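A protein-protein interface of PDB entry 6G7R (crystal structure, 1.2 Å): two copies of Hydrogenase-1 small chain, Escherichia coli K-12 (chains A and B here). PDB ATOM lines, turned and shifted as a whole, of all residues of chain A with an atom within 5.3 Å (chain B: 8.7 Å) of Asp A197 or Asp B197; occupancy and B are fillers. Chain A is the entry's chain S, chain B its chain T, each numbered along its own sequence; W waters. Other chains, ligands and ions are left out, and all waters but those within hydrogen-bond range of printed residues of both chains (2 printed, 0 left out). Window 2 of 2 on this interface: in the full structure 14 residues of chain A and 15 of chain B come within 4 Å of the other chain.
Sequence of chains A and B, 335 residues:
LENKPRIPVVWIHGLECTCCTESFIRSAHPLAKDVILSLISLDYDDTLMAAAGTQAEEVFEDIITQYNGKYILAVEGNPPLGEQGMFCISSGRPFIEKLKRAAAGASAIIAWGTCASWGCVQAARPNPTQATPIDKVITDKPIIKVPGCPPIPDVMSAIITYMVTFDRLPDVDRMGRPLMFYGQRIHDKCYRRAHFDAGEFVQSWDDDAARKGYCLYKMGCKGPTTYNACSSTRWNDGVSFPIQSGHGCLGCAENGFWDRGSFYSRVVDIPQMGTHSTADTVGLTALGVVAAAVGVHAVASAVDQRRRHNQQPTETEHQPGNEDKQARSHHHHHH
NH2 of Arg A193 lies within salt-bridge range of OD2 of Asp B197 (3.5 Å).
The guanidinium group of Arg B193 is in salt-bridge range of the side-chain carboxylate of Asp A197 (3.8 Å).
OD1 of Asp A197 sits close to OD1 of Asp B197 (2.4 Å).
O of His B187 lies within hydrogen-bond range of NH1 of Arg B193.
CB of Arg B193 touches CB of Arg A193 (3.9 Å).
Ala B194 touches Arg A193 (CB to NH1, 3.3 Å).
Ala A194 touches His B187 (CB to O, 3.7 Å).
Ala A194 touches Arg B193.
Of the printed residues of chain B, Arg A193 touches Arg B193, Ala B194 and Asp B197.
Of the printed residues of chain B, Asp A197 touches Arg B193 and Asp B197.
Of the printed residues of chain A, His B187 touches Ala A194 (3.7 Å).
Of the printed residues of chain A, Arg B193 touches Arg A193 (3.9 Å), Ala A194 (3.2 Å) and Asp A197 (3.8 Å).
Of chain A, only Arg A193 and Asp A197 come within 4 Å of Asp B197.
The nearest printed residue of chain B that does not touch Asp A197 is Phe B196 (6.3 Å).
Of the 13 printed residues of chain B, 4 touch a printed residue of chain A.
Printed residues of chain A that touch a printed residue of chain B: Arg A193, Ala A194 and Asp A197.
Hydrophobic or aromatic side chains of chain A within 4 Å of the printed part of chain B: Ala A194.
Arg B193 touches its own counterpart, Arg A193.
Arg A193 touches Ala B194, and with the chains exchanged Ala A194 touches Arg B193.
Arg A193 touches Asp B197, and with the chains exchanged Asp A197 touches Arg B193.
Asp A197 touches its own counterpart, Asp B197.
7 positions are printed for both chains.
Of the 7 pairs that touch across the chains among the printed residues, 6 have their exchanged pair printed and touching as well.
Water W1 bridges NH2 of Arg B193 (2.5 Å) and O of Ala A194 (2.8 Å).
Water W2 bridges O of Ala B194 (2.8 Å) and NH2 of Arg A193 (2.8 Å).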
ATOM      1  N   ARG A 193      28.118 -27.021 -29.749  1.00  0.00           N
ATOM      2  CA  ARG A 193      28.577 -26.570 -28.434  1.00  0.00           C
ATOM      3  C   ARG A 193      27.832 -27.255 -27.294  1.00  0.00           C
ATOM      4  O   ARG A 193      28.467 -27.455 -26.248  1.00  0.00           O
ATOM      5  CB  ARG A 193      28.466 -25.061 -28.289  1.00  0.00           C
ATOM      6  CG  ARG A 193      29.689 -24.279 -28.745  1.00  0.00           C
ATOM      7  CD  ARG A 193      30.916 -24.502 -27.875  1.00  0.00           C
ATOM      8  NE  ARG A 193      30.823 -24.025 -26.513  1.00  0.00           N
ATOM      9  CZ  ARG A 193      31.386 -22.914 -26.035  1.00  0.00           C
ATOM     10  NH1 ARG A 193      31.915 -22.023 -26.856  1.00  0.00           N
ATOM     11  NH2 ARG A 193      31.360 -22.706 -24.726  1.00  0.00           N
ATOM     12  N   ALA A 194      26.571 -27.630 -27.444  1.00  0.00           N
ATOM     13  CA  ALA A 194      25.898 -28.380 -26.405  1.00  0.00           C
ATOM     14  C   ALA A 194      26.715 -29.611 -26.020  1.00  0.00           C
ATOM     15  O   ALA A 194      26.795 -29.990 -24.838  1.00  0.00           O
ATOM     16  CB  ALA A 194      24.523 -28.791 -26.888  1.00  0.00           C
ATOM     17  N   HIS A 195      27.244 -30.283 -27.033  1.00  0.00           N
ATOM     18  CA  HIS A 195      28.004 -31.513 -26.806  1.00  0.00           C
ATOM     19  C   HIS A 195      29.353 -31.194 -26.156  1.00  0.00           C
ATOM     20  O   HIS A 195      29.766 -31.886 -25.227  1.00  0.00           O
ATOM     21  CB  HIS A 195      28.161 -32.282 -28.101  1.00  0.00           C
ATOM     22  CG  HIS A 195      26.840 -32.670 -28.702  1.00  0.00           C
ATOM     23  ND1 HIS A 195      25.920 -33.434 -28.019  1.00  0.00           N
ATOM     24  CD2 HIS A 195      26.286 -32.402 -29.910  1.00  0.00           C
ATOM     25  CE1 HIS A 195      24.861 -33.594 -28.812  1.00  0.00           C
ATOM     26  NE2 HIS A 195      25.068 -33.001 -29.980  1.00  0.00           N
ATOM     27  N   PHE A 196      30.052 -30.161 -26.629  1.00  0.00           N
ATOM     28  CA  PHE A 196      31.293 -29.730 -26.006  1.00  0.00           C
ATOM     29  C   PHE A 196      31.035 -29.498 -24.516  1.00  0.00           C
ATOM     30  O   PHE A 196      31.820 -29.972 -23.670  1.00  0.00           O
ATOM     31  CB  PHE A 196      31.774 -28.453 -26.685  1.00  0.00           C
ATOM     32  CG  PHE A 196      33.040 -27.874 -26.104  1.00  0.00           C
ATOM     33  CD1 PHE A 196      34.281 -28.334 -26.515  1.00  0.00           C
ATOM     34  CD2 PHE A 196      32.993 -26.882 -25.145  1.00  0.00           C
ATOM     35  CE1 PHE A 196      35.435 -27.788 -25.980  1.00  0.00           C
ATOM     36  CE2 PHE A 196      34.149 -26.323 -24.618  1.00  0.00           C
ATOM     37  CZ  PHE A 196      35.373 -26.776 -25.048  1.00  0.00           C
ATOM     38  N   ASP A 197      29.987 -28.760 -24.177  1.00  0.00           N
ATOM     39  CA  ASP A 197      29.704 -28.394 -22.790  1.00  0.00           C
ATOM     40  C   ASP A 197      29.449 -29.633 -21.942  1.00  0.00           C
ATOM     41  O   ASP A 197      29.751 -29.668 -20.746  1.00  0.00           O
ATOM     42  CB  ASP A 197      28.427 -27.574 -22.650  1.00  0.00           C
ATOM     43  CG  ASP A 197      28.164 -27.117 -21.222  1.00  0.00           C
ATOM     44  OD1 ASP A 197      28.987 -26.340 -20.701  1.00  0.00           O
ATOM     45  OD2 ASP A 197      27.184 -27.597 -20.604  1.00  0.00           O
ATOM     46  N   ALA A 198      28.819 -30.653 -22.555  1.00  0.00           N
ATOM     47  CA  ALA A 198      28.456 -31.892 -21.860  1.00  0.00           C
ATOM     48  C   ALA A 198      29.584 -32.928 -21.856  1.00  0.00           C
ATOM     49  O   ALA A 198      29.419 -34.001 -21.301  1.00  0.00           O
ATOM     50  CB  ALA A 198      27.240 -32.495 -22.508  1.00  0.00           C
ATOM     51  N   GLY A 199      30.690 -32.644 -22.496  1.00  0.00           N
ATOM     52  CA  GLY A 199      31.761 -33.645 -22.581  1.00  0.00           C
ATOM     53  C   GLY A 199      31.396 -34.800 -23.505  1.00  0.00           C
ATOM     54  O   GLY A 199      31.913 -35.902 -23.321  1.00  0.00           O
ATOM     55  N   HIS B 187      17.831 -27.212 -28.198  1.00  0.00           N
ATOM     56  CA  HIS B 187      18.917 -26.692 -27.374  1.00  0.00           C
ATOM     57  C   HIS B 187      20.145 -27.615 -27.371  1.00  0.00           C
ATOM     58  O   HIS B 187      21.216 -27.166 -26.975  1.00  0.00           O
ATOM     59  CB  HIS B 187      18.340 -26.478 -25.977  1.00  0.00           C
ATOM     60  CG  HIS B 187      19.218 -25.993 -24.891  1.00  0.00           C
ATOM     61  ND1 HIS B 187      19.562 -24.666 -24.738  1.00  0.00           N
ATOM     62  CD2 HIS B 187      19.660 -26.646 -23.790  1.00  0.00           C
ATOM     63  CE1 HIS B 187      20.210 -24.531 -23.603  1.00  0.00           C
ATOM     64  NE2 HIS B 187      20.298 -25.729 -22.989  1.00  0.00           N
ATOM     65  N   ARG B 192      23.553 -20.995 -30.592  1.00  0.00           N
ATOM     66  CA  ARG B 192      23.785 -20.007 -29.539  1.00  0.00           C
ATOM     67  C   ARG B 192      24.129 -20.648 -28.196  1.00  0.00           C
ATOM     68  O   ARG B 192      24.254 -19.920 -27.190  1.00  0.00           O
ATOM     69  CB  ARG B 192      22.604 -19.053 -29.385  1.00  0.00           C
ATOM     70  CG  ARG B 192      22.303 -18.316 -30.677  1.00  0.00           C
ATOM     71  CD  ARG B 192      21.230 -17.263 -30.541  1.00  0.00           C
ATOM     72  NE  ARG B 192      21.003 -16.586 -31.807  1.00  0.00           N
ATOM     73  CZ  ARG B 192      20.448 -15.395 -31.984  1.00  0.00           C
ATOM     74  NH1 ARG B 192      20.081 -14.649 -30.943  1.00  0.00           N
ATOM     75  NH2 ARG B 192      20.268 -14.958 -33.236  1.00  0.00           N
ATOM     76  N   ARG B 193      24.419 -21.941 -28.186  1.00  0.00           N
ATOM     77  CA  ARG B 193      24.756 -22.618 -26.930  1.00  0.00           C
ATOM     78  C   ARG B 193      26.045 -22.065 -26.308  1.00  0.00           C
ATOM     79  O   ARG B 193      26.157 -22.073 -25.077  1.00  0.00           O
ATOM     80  CB  ARG B 193      24.895 -24.133 -27.112  1.00  0.00           C
ATOM     81  CG  ARG B 193      23.691 -24.949 -26.669  1.00  0.00           C
ATOM     82  CD  ARG B 193      23.218 -24.721 -25.232  1.00  0.00           C
ATOM     83  NE  ARG B 193      23.859 -25.526 -24.203  1.00  0.00           N
ATOM     84  CZ  ARG B 193      23.585 -26.808 -23.944  1.00  0.00           C
ATOM     85  NH1 ARG B 193      22.679 -27.460 -24.652  1.00  0.00           N
ATOM     86  NH2 ARG B 193      24.246 -27.431 -22.983  1.00  0.00           N
ATOM     87  N   ALA B 194      27.015 -21.600 -27.099  1.00  0.00           N
ATOM     88  CA  ALA B 194      28.242 -20.997 -26.503  1.00  0.00           C
ATOM     89  C   ALA B 194      27.825 -19.867 -25.551  1.00  0.00           C
ATOM     90  O   ALA B 194      28.428 -19.652 -24.515  1.00  0.00           O
ATOM     91  CB  ALA B 194      29.115 -20.442 -27.593  1.00  0.00           C
ATOM     92  N   HIS B 195      26.864 -19.058 -25.982  1.00  0.00           N
ATOM     93  CA  HIS B 195      26.404 -17.920 -25.202  1.00  0.00           C
ATOM     94  C   HIS B 195      25.634 -18.397 -23.960  1.00  0.00           C
ATOM     95  O   HIS B 195      25.838 -17.864 -22.876  1.00  0.00           O
ATOM     96  CB  HIS B 195      25.575 -16.990 -26.056  1.00  0.00           C
ATOM     97  CG  HIS B 195      26.325 -16.469 -27.232  1.00  0.00           C
ATOM     98  ND1 HIS B 195      27.519 -15.791 -27.114  1.00  0.00           N
ATOM     99  CD2 HIS B 195      26.064 -16.524 -28.568  1.00  0.00           C
ATOM    100  CE1 HIS B 195      27.961 -15.474 -28.339  1.00  0.00           C
ATOM    101  NE2 HIS B 195      27.054 -15.878 -29.251  1.00  0.00           N
ATOM    102  N   PHE B 196      24.751 -19.387 -24.114  1.00  0.00           N
ATOM    103  CA  PHE B 196      24.064 -19.966 -22.965  1.00  0.00           C
ATOM    104  C   PHE B 196      25.089 -20.383 -21.919  1.00  0.00           C
ATOM    105  O   PHE B 196      24.934 -20.081 -20.705  1.00  0.00           O
ATOM    106  CB  PHE B 196      23.210 -21.148 -23.417  1.00  0.00           C
ATOM    107  CG  PHE B 196      22.478 -21.838 -22.301  1.00  0.00           C
ATOM    108  CD1 PHE B 196      21.244 -21.389 -21.855  1.00  0.00           C
ATOM    109  CD2 PHE B 196      23.024 -22.952 -21.694  1.00  0.00           C
ATOM    110  CE1 PHE B 196      20.578 -22.058 -20.842  1.00  0.00           C
ATOM    111  CE2 PHE B 196      22.363 -23.617 -20.676  1.00  0.00           C
ATOM    112  CZ  PHE B 196      21.132 -23.167 -20.255  1.00  0.00           C
ATOM    113  N   ASP B 197      26.108 -21.110 -22.345  1.00  0.00           N
ATOM    114  CA  ASP B 197      27.145 -21.674 -21.453  1.00  0.00           C
ATOM    115  C   ASP B 197      27.871 -20.566 -20.715  1.00  0.00           C
ATOM    116  O   ASP B 197      28.290 -20.724 -19.544  1.00  0.00           O
ATOM    117  CB  ASP B 197      28.271 -22.392 -22.204  1.00  0.00           C
ATOM    118  CG  ASP B 197      29.310 -23.030 -21.285  1.00  0.00           C
ATOM    119  OD1 ASP B 197      28.914 -23.917 -20.510  1.00  0.00           O
ATOM    120  OD2 ASP B 197      30.494 -22.604 -21.306  1.00  0.00           O
ATOM    121  N   ALA B 198      28.097 -19.442 -21.404  1.00  0.00           N
ATOM    122  CA  ALA B 198      28.875 -18.303 -20.882  1.00  0.00           C
ATOM    123  C   ALA B 198      28.016 -17.319 -20.077  1.00  0.00           C
ATOM    124  O   ALA B 198      28.507 -16.313 -19.585  1.00  0.00           O
ATOM    125  CB  ALA B 198      29.539 -17.591 -22.045  1.00  0.00           C
ATOM    126  N   GLY B 199      26.722 -17.550 -20.014  1.00  0.00           N
ATOM    127  CA  GLY B 199      25.841 -16.603 -19.349  1.00  0.00           C
ATOM    128  C   GLY B 199      25.632 -15.318 -20.130  1.00  0.00           C
ATOM    129  O   GLY B 199      25.395 -14.271 -19.529  1.00  0.00           O
ATOM    130  N   GLU B 200      25.668 -15.408 -21.443  1.00  0.00           N
ATOM    131  CA  GLU B 200      25.586 -14.283 -22.348  1.00  0.00           C
ATOM    132  C   GLU B 200      24.192 -14.285 -22.985  1.00  0.00           C
ATOM    133  O   GLU B 200      23.902 -15.084 -23.911  1.00  0.00           O
ATOM    134  CB  GLU B 200      26.660 -14.406 -23.418  1.00  0.00           C
ATOM    135  CG  GLU B 200      28.034 -14.068 -22.866  1.00  0.00           C
ATOM    136  CD  GLU B 200      29.194 -14.382 -23.778  1.00  0.00           C
ATOM    137  OE1 GLU B 200      30.330 -13.991 -23.390  1.00  0.00           O
ATOM    138  OE2 GLU B 200      29.012 -15.027 -24.844  1.00  0.00           O
ATOM    139  N   PHE B 201      23.323 -13.386 -22.480  1.00  0.00           N
ATOM    140  CA  PHE B 201      21.893 -13.439 -22.778  1.00  0.00           C
ATOM    141  C   PHE B 201      21.372 -12.114 -23.313  1.00  0.00           C
ATOM    142  O   PHE B 201      21.736 -11.060 -22.797  1.00  0.00           O
ATOM    143  CB  PHE B 201      21.089 -13.781 -21.526  1.00  0.00           C
ATOM    144  CG  PHE B 201      21.444 -15.104 -20.907  1.00  0.00           C
ATOM    145  CD1 PHE B 201      21.121 -16.278 -21.553  1.00  0.00           C
ATOM    146  CD2 PHE B 201      22.051 -15.179 -19.673  1.00  0.00           C
ATOM    147  CE1 PHE B 201      21.447 -17.494 -20.997  1.00  0.00           C
ATOM    148  CE2 PHE B 201      22.348 -16.405 -19.096  1.00  0.00           C
ATOM    149  CZ  PHE B 201      22.053 -17.562 -19.764  1.00  0.00           C
ATOM    150  N   CYS B 215      22.211 -15.720 -26.518  1.00  0.00           N
ATOM    151  CA  CYS B 215      21.200 -16.705 -26.230  1.00  0.00           C
ATOM    152  C   CYS B 215      19.899 -16.011 -25.793  1.00  0.00           C
ATOM    153  O   CYS B 215      19.904 -14.971 -25.127  1.00  0.00           O
ATOM    154  CB  CYS B 215      21.734 -17.642 -25.142  1.00  0.00           C
ATOM    155  SG  CYS B 215      20.517 -18.754 -24.398  1.00  0.00           S
ATOM    156  N   TYR B 217      17.446 -17.481 -23.882  1.00  0.00           N
ATOM    157  CA  TYR B 217      16.851 -18.112 -22.696  1.00  0.00           C
ATOM    158  C   TYR B 217      16.063 -17.117 -21.842  1.00  0.00           C
ATOM    159  O   TYR B 217      14.958 -17.439 -21.390  1.00  0.00           O
ATOM    160  CB  TYR B 217      17.968 -18.774 -21.893  1.00  0.00           C
ATOM    161  CG  TYR B 217      17.560 -19.246 -20.533  1.00  0.00           C
ATOM    162  CD1 TYR B 217      16.798 -20.386 -20.362  1.00  0.00           C
ATOM    163  CD2 TYR B 217      17.972 -18.527 -19.416  1.00  0.00           C
ATOM    164  CE1 TYR B 217      16.426 -20.780 -19.097  1.00  0.00           C
ATOM    165  CE2 TYR B 217      17.567 -18.890 -18.151  1.00  0.00           C
ATOM    166  CZ  TYR B 217      16.800 -20.027 -18.008  1.00  0.00           C
ATOM    167  OH  TYR B 217      16.406 -20.445 -16.801  1.00  0.00           O
HETATM  168  O   HOH W   1      24.792 -29.906 -22.955  1.00  0.00           O
HETATM  169  O   HOH W   2      31.139 -19.962 -24.123  1.00  0.00           O
